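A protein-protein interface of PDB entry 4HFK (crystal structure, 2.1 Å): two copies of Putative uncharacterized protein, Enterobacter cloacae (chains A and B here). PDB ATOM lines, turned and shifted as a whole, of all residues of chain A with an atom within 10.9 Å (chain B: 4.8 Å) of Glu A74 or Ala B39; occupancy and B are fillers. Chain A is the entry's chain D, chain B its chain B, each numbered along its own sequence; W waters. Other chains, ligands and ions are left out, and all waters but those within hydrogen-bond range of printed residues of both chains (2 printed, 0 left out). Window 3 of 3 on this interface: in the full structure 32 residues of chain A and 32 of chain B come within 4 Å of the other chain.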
ATOM      1  N   LYS A  69       8.721 -15.302  15.984  1.00  0.00           N
ATOM      2  CA  LYS A  69       9.363 -15.632  17.245  1.00  0.00           C
ATOM      3  C   LYS A  69       8.294 -16.077  18.225  1.00  0.00           C
ATOM      4  O   LYS A  69       7.321 -15.368  18.470  1.00  0.00           O
ATOM      5  CB  LYS A  69      10.130 -14.432  17.792  1.00  0.00           C
ATOM      6  CG  LYS A  69      11.618 -14.473  17.483  1.00  0.00           C
ATOM      7  CD  LYS A  69      12.235 -13.082  17.517  1.00  0.00           C
ATOM      8  CE  LYS A  69      13.730 -13.147  17.238  1.00  0.00           C
ATOM      9  NZ  LYS A  69      14.310 -11.804  16.977  1.00  0.00           N
ATOM     10  N   VAL A  70       8.476 -17.266  18.779  1.00  0.00           N
ATOM     11  CA  VAL A  70       7.482 -17.855  19.659  1.00  0.00           C
ATOM     12  C   VAL A  70       8.175 -18.235  20.980  1.00  0.00           C
ATOM     13  O   VAL A  70       9.330 -18.684  20.971  1.00  0.00           O
ATOM     14  CB  VAL A  70       6.809 -19.033  18.924  1.00  0.00           C
ATOM     15  CG1 VAL A  70       7.186 -20.351  19.517  1.00  0.00           C
ATOM     16  CG2 VAL A  70       5.305 -18.840  18.859  1.00  0.00           C
ATOM     17  N   GLY A  71       7.514 -17.999  22.116  1.00  0.00           N
ATOM     18  CA  GLY A  71       8.164 -18.188  23.404  1.00  0.00           C
ATOM     19  C   GLY A  71       7.312 -18.804  24.506  1.00  0.00           C
ATOM     20  O   GLY A  71       6.106 -18.986  24.346  1.00  0.00           O
ATOM     21  N   GLY A  72       7.959 -19.118  25.628  1.00  0.00           N
ATOM     22  CA  GLY A  72       7.328 -19.768  26.768  1.00  0.00           C
ATOM     23  C   GLY A  72       8.184 -19.579  28.013  1.00  0.00           C
ATOM     24  O   GLY A  72       9.148 -18.795  27.991  1.00  0.00           O
ATOM     25  N   THR A  73       7.843 -20.274  29.102  1.00  0.00           N
ATOM     26  CA  THR A  73       8.614 -20.142  30.333  1.00  0.00           C
ATOM     27  C   THR A  73       9.997 -20.776  30.198  1.00  0.00           C
ATOM     28  O   THR A  73      10.918 -20.387  30.911  1.00  0.00           O
ATOM     29  CB  THR A  73       7.893 -20.724  31.567  1.00  0.00           C
ATOM     30  OG1 THR A  73       7.791 -22.147  31.437  1.00  0.00           O
ATOM     31  CG2 THR A  73       6.499 -20.103  31.725  1.00  0.00           C
ATOM     32  N   GLU A  74      10.141 -21.743  29.291  1.00  0.00           N
ATOM     33  CA  GLU A  74      11.451 -22.350  29.016  1.00  0.00           C
ATOM     34  C   GLU A  74      12.274 -21.433  28.121  1.00  0.00           C
ATOM     35  O   GLU A  74      11.704 -20.633  27.373  1.00  0.00           O
ATOM     36  CB  GLU A  74      11.298 -23.726  28.358  1.00  0.00           C
ATOM     37  CG  GLU A  74      10.753 -24.802  29.290  1.00  0.00           C
ATOM     38  CD  GLU A  74      11.674 -25.077  30.464  1.00  0.00           C
ATOM     39  OE1 GLU A  74      12.826 -25.499  30.234  1.00  0.00           O
ATOM     40  OE2 GLU A  74      11.247 -24.868  31.617  1.00  0.00           O
ATOM     41  N   PRO A  75      13.619 -21.536  28.194  1.00  0.00           N
ATOM     42  CA  PRO A  75      14.467 -20.584  27.460  1.00  0.00           C
ATOM     43  C   PRO A  75      14.428 -20.750  25.938  1.00  0.00           C
ATOM     44  O   PRO A  75      14.682 -19.770  25.246  1.00  0.00           O
ATOM     45  CB  PRO A  75      15.891 -20.904  27.953  1.00  0.00           C
ATOM     46  CG  PRO A  75      15.734 -21.779  29.145  1.00  0.00           C
ATOM     47  CD  PRO A  75      14.416 -22.478  29.002  1.00  0.00           C
ATOM     48  N   GLY A  76      14.130 -21.944  25.427  1.00  0.00           N
ATOM     49  CA  GLY A  76      14.190 -22.184  23.988  1.00  0.00           C
ATOM     50  C   GLY A  76      13.240 -21.403  23.077  1.00  0.00           C
ATOM     51  O   GLY A  76      12.545 -20.472  23.503  1.00  0.00           O
ATOM     52  N   HIS A  77      13.224 -21.783  21.802  1.00  0.00           N
ATOM     53  CA  HIS A  77      12.410 -21.095  20.806  1.00  0.00           C
ATOM     54  C   HIS A  77      11.128 -21.856  20.456  1.00  0.00           C
ATOM     55  O   HIS A  77      10.400 -21.439  19.548  1.00  0.00           O
ATOM     56  CB  HIS A  77      13.220 -20.856  19.524  1.00  0.00           C
ATOM     57  CG  HIS A  77      14.469 -20.056  19.735  1.00  0.00           C
ATOM     58  ND1 HIS A  77      14.465 -18.804  20.314  1.00  0.00           N
ATOM     59  CD2 HIS A  77      15.764 -20.332  19.446  1.00  0.00           C
ATOM     60  CE1 HIS A  77      15.702 -18.344  20.369  1.00  0.00           C
ATOM     61  NE2 HIS A  77      16.509 -19.251  19.845  1.00  0.00           N
ATOM     62  N   TYR A  78      10.866 -22.966  21.158  1.00  0.00           N
ATOM     63  CA  TYR A  78       9.651 -23.761  20.945  1.00  0.00           C
ATOM     64  C   TYR A  78       9.382 -24.040  19.464  1.00  0.00           C
ATOM     65  O   TYR A  78       8.246 -23.883  18.997  1.00  0.00           O
ATOM     66  CB  TYR A  78       8.442 -23.029  21.538  1.00  0.00           C
ATOM     67  CG  TYR A  78       8.424 -23.032  23.042  1.00  0.00           C
ATOM     68  CD1 TYR A  78       7.614 -23.914  23.740  1.00  0.00           C
ATOM     69  CD2 TYR A  78       9.226 -22.163  23.763  1.00  0.00           C
ATOM     70  CE1 TYR A  78       7.593 -23.918  25.118  1.00  0.00           C
ATOM     71  CE2 TYR A  78       9.217 -22.162  25.140  1.00  0.00           C
ATOM     72  CZ  TYR A  78       8.398 -23.038  25.813  1.00  0.00           C
ATOM     73  OH  TYR A  78       8.384 -23.032  27.196  1.00  0.00           O
ATOM     74  N   GLN A  79      10.425 -24.419  18.723  1.00  0.00           N
ATOM     75  CA  GLN A  79      10.283 -24.655  17.285  1.00  0.00           C
ATOM     76  C   GLN A  79       9.347 -25.813  16.979  1.00  0.00           C
ATOM     77  O   GLN A  79       8.561 -25.754  16.022  1.00  0.00           O
ATOM     78  CB  GLN A  79      11.650 -24.919  16.640  1.00  0.00           C
ATOM     79  CG  GLN A  79      12.641 -23.770  16.781  1.00  0.00           C
ATOM     80  CD  GLN A  79      12.475 -22.709  15.702  1.00  0.00           C
ATOM     81  OE1 GLN A  79      11.356 -22.334  15.340  1.00  0.00           O
ATOM     82  NE2 GLN A  79      13.594 -22.234  15.169  1.00  0.00           N
ATOM     83  N   ILE A  80       9.441 -26.877  17.767  1.00  0.00           N
ATOM     84  CA  ILE A  80       8.646 -28.070  17.488  1.00  0.00           C
ATOM     85  C   ILE A  80       7.154 -27.734  17.655  1.00  0.00           C
ATOM     86  O   ILE A  80       6.320 -28.135  16.836  1.00  0.00           O
ATOM     87  CB  ILE A  80       9.065 -29.251  18.385  1.00  0.00           C
ATOM     88  CG1 ILE A  80      10.427 -29.793  17.943  1.00  0.00           C
ATOM     89  CG2 ILE A  80       8.008 -30.359  18.377  1.00  0.00           C
ATOM     90  CD1 ILE A  80      10.438 -30.394  16.556  1.00  0.00           C
ATOM     91  N   LEU A  81       6.827 -26.975  18.699  1.00  0.00           N
ATOM     92  CA  LEU A  81       5.463 -26.459  18.844  1.00  0.00           C
ATOM     93  C   LEU A  81       5.091 -25.599  17.634  1.00  0.00           C
ATOM     94  O   LEU A  81       4.052 -25.819  17.014  1.00  0.00           O
ATOM     95  CB  LEU A  81       5.314 -25.662  20.142  1.00  0.00           C
ATOM     96  CG  LEU A  81       3.999 -24.911  20.403  1.00  0.00           C
ATOM     97  CD1 LEU A  81       2.776 -25.798  20.249  1.00  0.00           C
ATOM     98  CD2 LEU A  81       4.018 -24.304  21.805  1.00  0.00           C
ATOM     99  N   LYS A  82       5.954 -24.641  17.291  1.00  0.00           N
ATOM    100  CA  LYS A  82       5.733 -23.766  16.132  1.00  0.00           C
ATOM    101  C   LYS A  82       5.416 -24.534  14.836  1.00  0.00           C
ATOM    102  O   LYS A  82       4.546 -24.119  14.066  1.00  0.00           O
ATOM    103  CB  LYS A  82       6.940 -22.849  15.905  1.00  0.00           C
ATOM    104  CG  LYS A  82       6.710 -21.810  14.798  1.00  0.00           C
ATOM    105  CD  LYS A  82       8.000 -21.091  14.375  1.00  0.00           C
ATOM    106  CE  LYS A  82       8.672 -20.383  15.534  1.00  0.00           C
ATOM    107  NZ  LYS A  82      10.057 -19.913  15.163  1.00  0.00           N
ATOM    108  N   LEU A  85       1.803 -25.424  14.907  1.00  0.00           N
ATOM    109  CA  LEU A  85       0.955 -24.241  14.778  1.00  0.00           C
ATOM    110  C   LEU A  85       0.922 -23.785  13.315  1.00  0.00           C
ATOM    111  O   LEU A  85      -0.131 -23.432  12.778  1.00  0.00           O
ATOM    112  CB  LEU A  85       1.466 -23.111  15.683  1.00  0.00           C
ATOM    113  CG  LEU A  85       1.560 -23.421  17.182  1.00  0.00           C
ATOM    114  CD1 LEU A  85       1.994 -22.184  17.959  1.00  0.00           C
ATOM    115  CD2 LEU A  85       0.216 -23.931  17.698  1.00  0.00           C
ATOM    116  N   GLU B  35      15.442 -30.818  23.922  1.00  0.00           N
ATOM    117  CA  GLU B  35      14.948 -29.829  24.880  1.00  0.00           C
ATOM    118  C   GLU B  35      13.771 -29.040  24.288  1.00  0.00           C
ATOM    119  O   GLU B  35      12.787 -28.772  24.976  1.00  0.00           O
ATOM    120  CB  GLU B  35      16.071 -28.886  25.333  1.00  0.00           C
ATOM    121  CG  GLU B  35      17.193 -29.603  26.085  1.00  0.00           C
ATOM    122  CD  GLU B  35      18.413 -28.723  26.353  1.00  0.00           C
ATOM    123  OE1 GLU B  35      18.409 -27.530  25.956  1.00  0.00           O
ATOM    124  OE2 GLU B  35      19.381 -29.232  26.965  1.00  0.00           O
ATOM    125  N   ASP B  36      13.879 -28.676  23.011  1.00  0.00           N
ATOM    126  CA  ASP B  36      12.812 -27.943  22.330  1.00  0.00           C
ATOM    127  C   ASP B  36      11.517 -28.782  22.267  1.00  0.00           C
ATOM    128  O   ASP B  36      10.422 -28.307  22.605  1.00  0.00           O
ATOM    129  CB  ASP B  36      13.288 -27.541  20.929  1.00  0.00           C
ATOM    130  CG  ASP B  36      12.288 -26.658  20.189  1.00  0.00           C
ATOM    131  OD1 ASP B  36      11.100 -27.038  20.087  1.00  0.00           O
ATOM    132  OD2 ASP B  36      12.692 -25.580  19.691  1.00  0.00           O
ATOM    133  N   ALA B  37      11.651 -30.036  21.847  1.00  0.00           N
ATOM    134  CA  ALA B  37      10.507 -30.927  21.739  1.00  0.00           C
ATOM    135  C   ALA B  37       9.846 -31.172  23.104  1.00  0.00           C
ATOM    136  O   ALA B  37       8.616 -31.241  23.197  1.00  0.00           O
ATOM    137  CB  ALA B  37      10.918 -32.243  21.088  1.00  0.00           C
ATOM    138  N   ASP B  38      10.644 -31.302  24.163  1.00  0.00           N
ATOM    139  CA  ASP B  38      10.071 -31.525  25.492  1.00  0.00           C
ATOM    140  C   ASP B  38       9.435 -30.256  26.077  1.00  0.00           C
ATOM    141  O   ASP B  38       8.454 -30.335  26.821  1.00  0.00           O
ATOM    142  CB  ASP B  38      11.121 -32.083  26.460  1.00  0.00           C
ATOM    143  CG  ASP B  38      11.524 -33.514  26.127  1.00  0.00           C
ATOM    144  OD1 ASP B  38      10.806 -34.188  25.346  1.00  0.00           O
ATOM    145  OD2 ASP B  38      12.560 -33.974  26.658  1.00  0.00           O
ATOM    146  N   ALA B  39      10.000 -29.093  25.756  1.00  0.00           N
ATOM    147  CA  ALA B  39       9.396 -27.833  26.178  1.00  0.00           C
ATOM    148  C   ALA B  39       8.082 -27.666  25.423  1.00  0.00           C
ATOM    149  O   ALA B  39       7.069 -27.254  25.987  1.00  0.00           O
ATOM    150  CB  ALA B  39      10.322 -26.667  25.894  1.00  0.00           C
ATOM    151  N   SER B  40       8.108 -27.996  24.140  1.00  0.00           N
ATOM    152  CA  SER B  40       6.906 -27.943  23.320  1.00  0.00           C
ATOM    153  C   SER B  40       5.823 -28.876  23.865  1.00  0.00           C
ATOM    154  O   SER B  40       4.658 -28.473  24.007  1.00  0.00           O
ATOM    155  CB  SER B  40       7.247 -28.298  21.870  1.00  0.00           C
ATOM    156  OG  SER B  40       8.125 -27.325  21.319  1.00  0.00           O
ATOM    157  N   ALA B  41       6.210 -30.107  24.192  1.00  0.00           N
ATOM    158  CA  ALA B  41       5.274 -31.080  24.748  1.00  0.00           C
ATOM    159  C   ALA B  41       4.642 -30.550  26.039  1.00  0.00           C
ATOM    160  O   ALA B  41       3.450 -30.754  26.292  1.00  0.00           O
ATOM    161  CB  ALA B  41       5.984 -32.419  25.001  1.00  0.00           C
ATOM    162  N   ALA B  42       5.433 -29.858  26.857  1.00  0.00           N
ATOM    163  CA  ALA B  42       4.913 -29.349  28.132  1.00  0.00           C
ATOM    164  C   ALA B  42       3.855 -28.260  27.928  1.00  0.00           C
ATOM    165  O   ALA B  42       3.052 -27.997  28.826  1.00  0.00           O
ATOM    166  CB  ALA B  42       6.053 -28.855  29.053  1.00  0.00           C
ATOM    167  N   ALA B  43       3.855 -27.620  26.760  1.00  0.00           N
ATOM    168  CA  ALA B  43       2.817 -26.629  26.462  1.00  0.00           C
ATOM    169  C   ALA B  43       1.494 -27.328  26.166  1.00  0.00           C
ATOM    170  O   ALA B  43       0.432 -26.863  26.587  1.00  0.00           O
ATOM    171  CB  ALA B  43       3.217 -25.747  25.295  1.00  0.00           C
HETATM  172  O   HOH W   1       7.435 -25.551  28.101  1.00  0.00           O
HETATM  173  O   HOH W   2      14.555 -24.121  20.881  1.00  0.00           O
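The backbone NH (N) of Gln A79 lies within hydrogen-bond range of the side-chain carboxylate (OD2) of Asp B36.
The side-chain carboxylate (OD1) of Asp B36 is in hydrogen-bond range of the backbone NH (N) of Ile A80 (2.9 Å).
The side-chain hydroxyl (OG) of Ser B40 is in hydrogen-bond range of the backbone NH (N) of Leu A81 (2.9 Å).
The backbone carbonyl oxygen (O) of Asp B36 is in hydrogen-bond range of the side-chain hydroxyl (OG) of Ser B40 (2.8 Å).
OH of Tyr A78 lies within hydrogen-bond range of N of Thr A73, 3.4 Å away.
The side-chain hydroxyl (OH) of Tyr A78 is in hydrogen-bond range of the backbone NH (N) of Glu A74 (3.0 Å).
The side-chain amino group (NZ) of Lys A82 lies within hydrogen-bond range of the side-chain amide oxygen (OE1) of Gln A79 (2.8 Å).
Glu A74 touches Ala B39.
Asp B36 touches Tyr A78.
Tyr A78 touches Ala B39.
Ser B40 touches Tyr A78.
CG1 of Ile A80 touches CA of Ala B37 (3.96 Å).
Ile A80 touches Ser B40 (CB to OG, 3.6 Å).
Leu A81 touches Ala B43 (CD2 to CB, 3.9 Å).
Of chain B, only Ala B39 comes within 4 Å of Glu A74.
Ala B39 touches two residues of chain A.
Of chain A, only Tyr A78 (3.5 Å), Gln A79 (2.7 Å) and Ile A80 (2.9 Å) come within 4 Å of Asp B36.
Ala B37 touches one residue of chain A.
No residue of chain A comes within 4 Å of Asp B38.
Of chain A, only Leu A81 comes within 4 Å of Ala B43.
Of the printed residues of chain B, Leu A81 touches Ser B40 and Ala B43.
Printed residues of chain B within 4 Å of Gln A79: Asp B36 (2.7 Å).
Of the printed residues of chain B, Tyr A78 touches Asp B36 (3.5 Å), Ala B39 (3.5 Å) and Ser B40 (3.9 Å).
Of the printed residues of chain B, Ile A80 touches Asp B36 (2.9 Å), Ala B37 (3.96 Å) and Ser B40 (3.6 Å).
The nearest residue of chain A that does not touch Ala B39 is Leu A81 (6.0 Å).
The nearest printed residue of chain B that does not touch Ile A80 is Ala B41 (6.1 Å).
Of the 15 printed residues of chain A, 5 touch a printed residue of chain B.
Printed residues of chain A that touch a printed residue of chain B: Glu A74, Tyr A78, Gln A79, Ile A80 and Leu A81.
Hydrophobic or aromatic side chains of chain B that line the printed part of chain A: Ala B39 and Ala B43.
Among the printed residues, no Asp or Glu carboxylate lies within 4 Å of a Lys or Arg side-chain nitrogen of the other chain.
No position is printed for both chains.
Water W2 lies within hydrogen-bond range of OD2 of Asp B36 (2.6 Å) and N of His A77 (2.8 Å).
Water W1 bridges the backbone carbonyl oxygen (O) of Ala B39 (2.7 Å) and the side-chain hydroxyl (OH) of Tyr A78 (2.8 Å).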
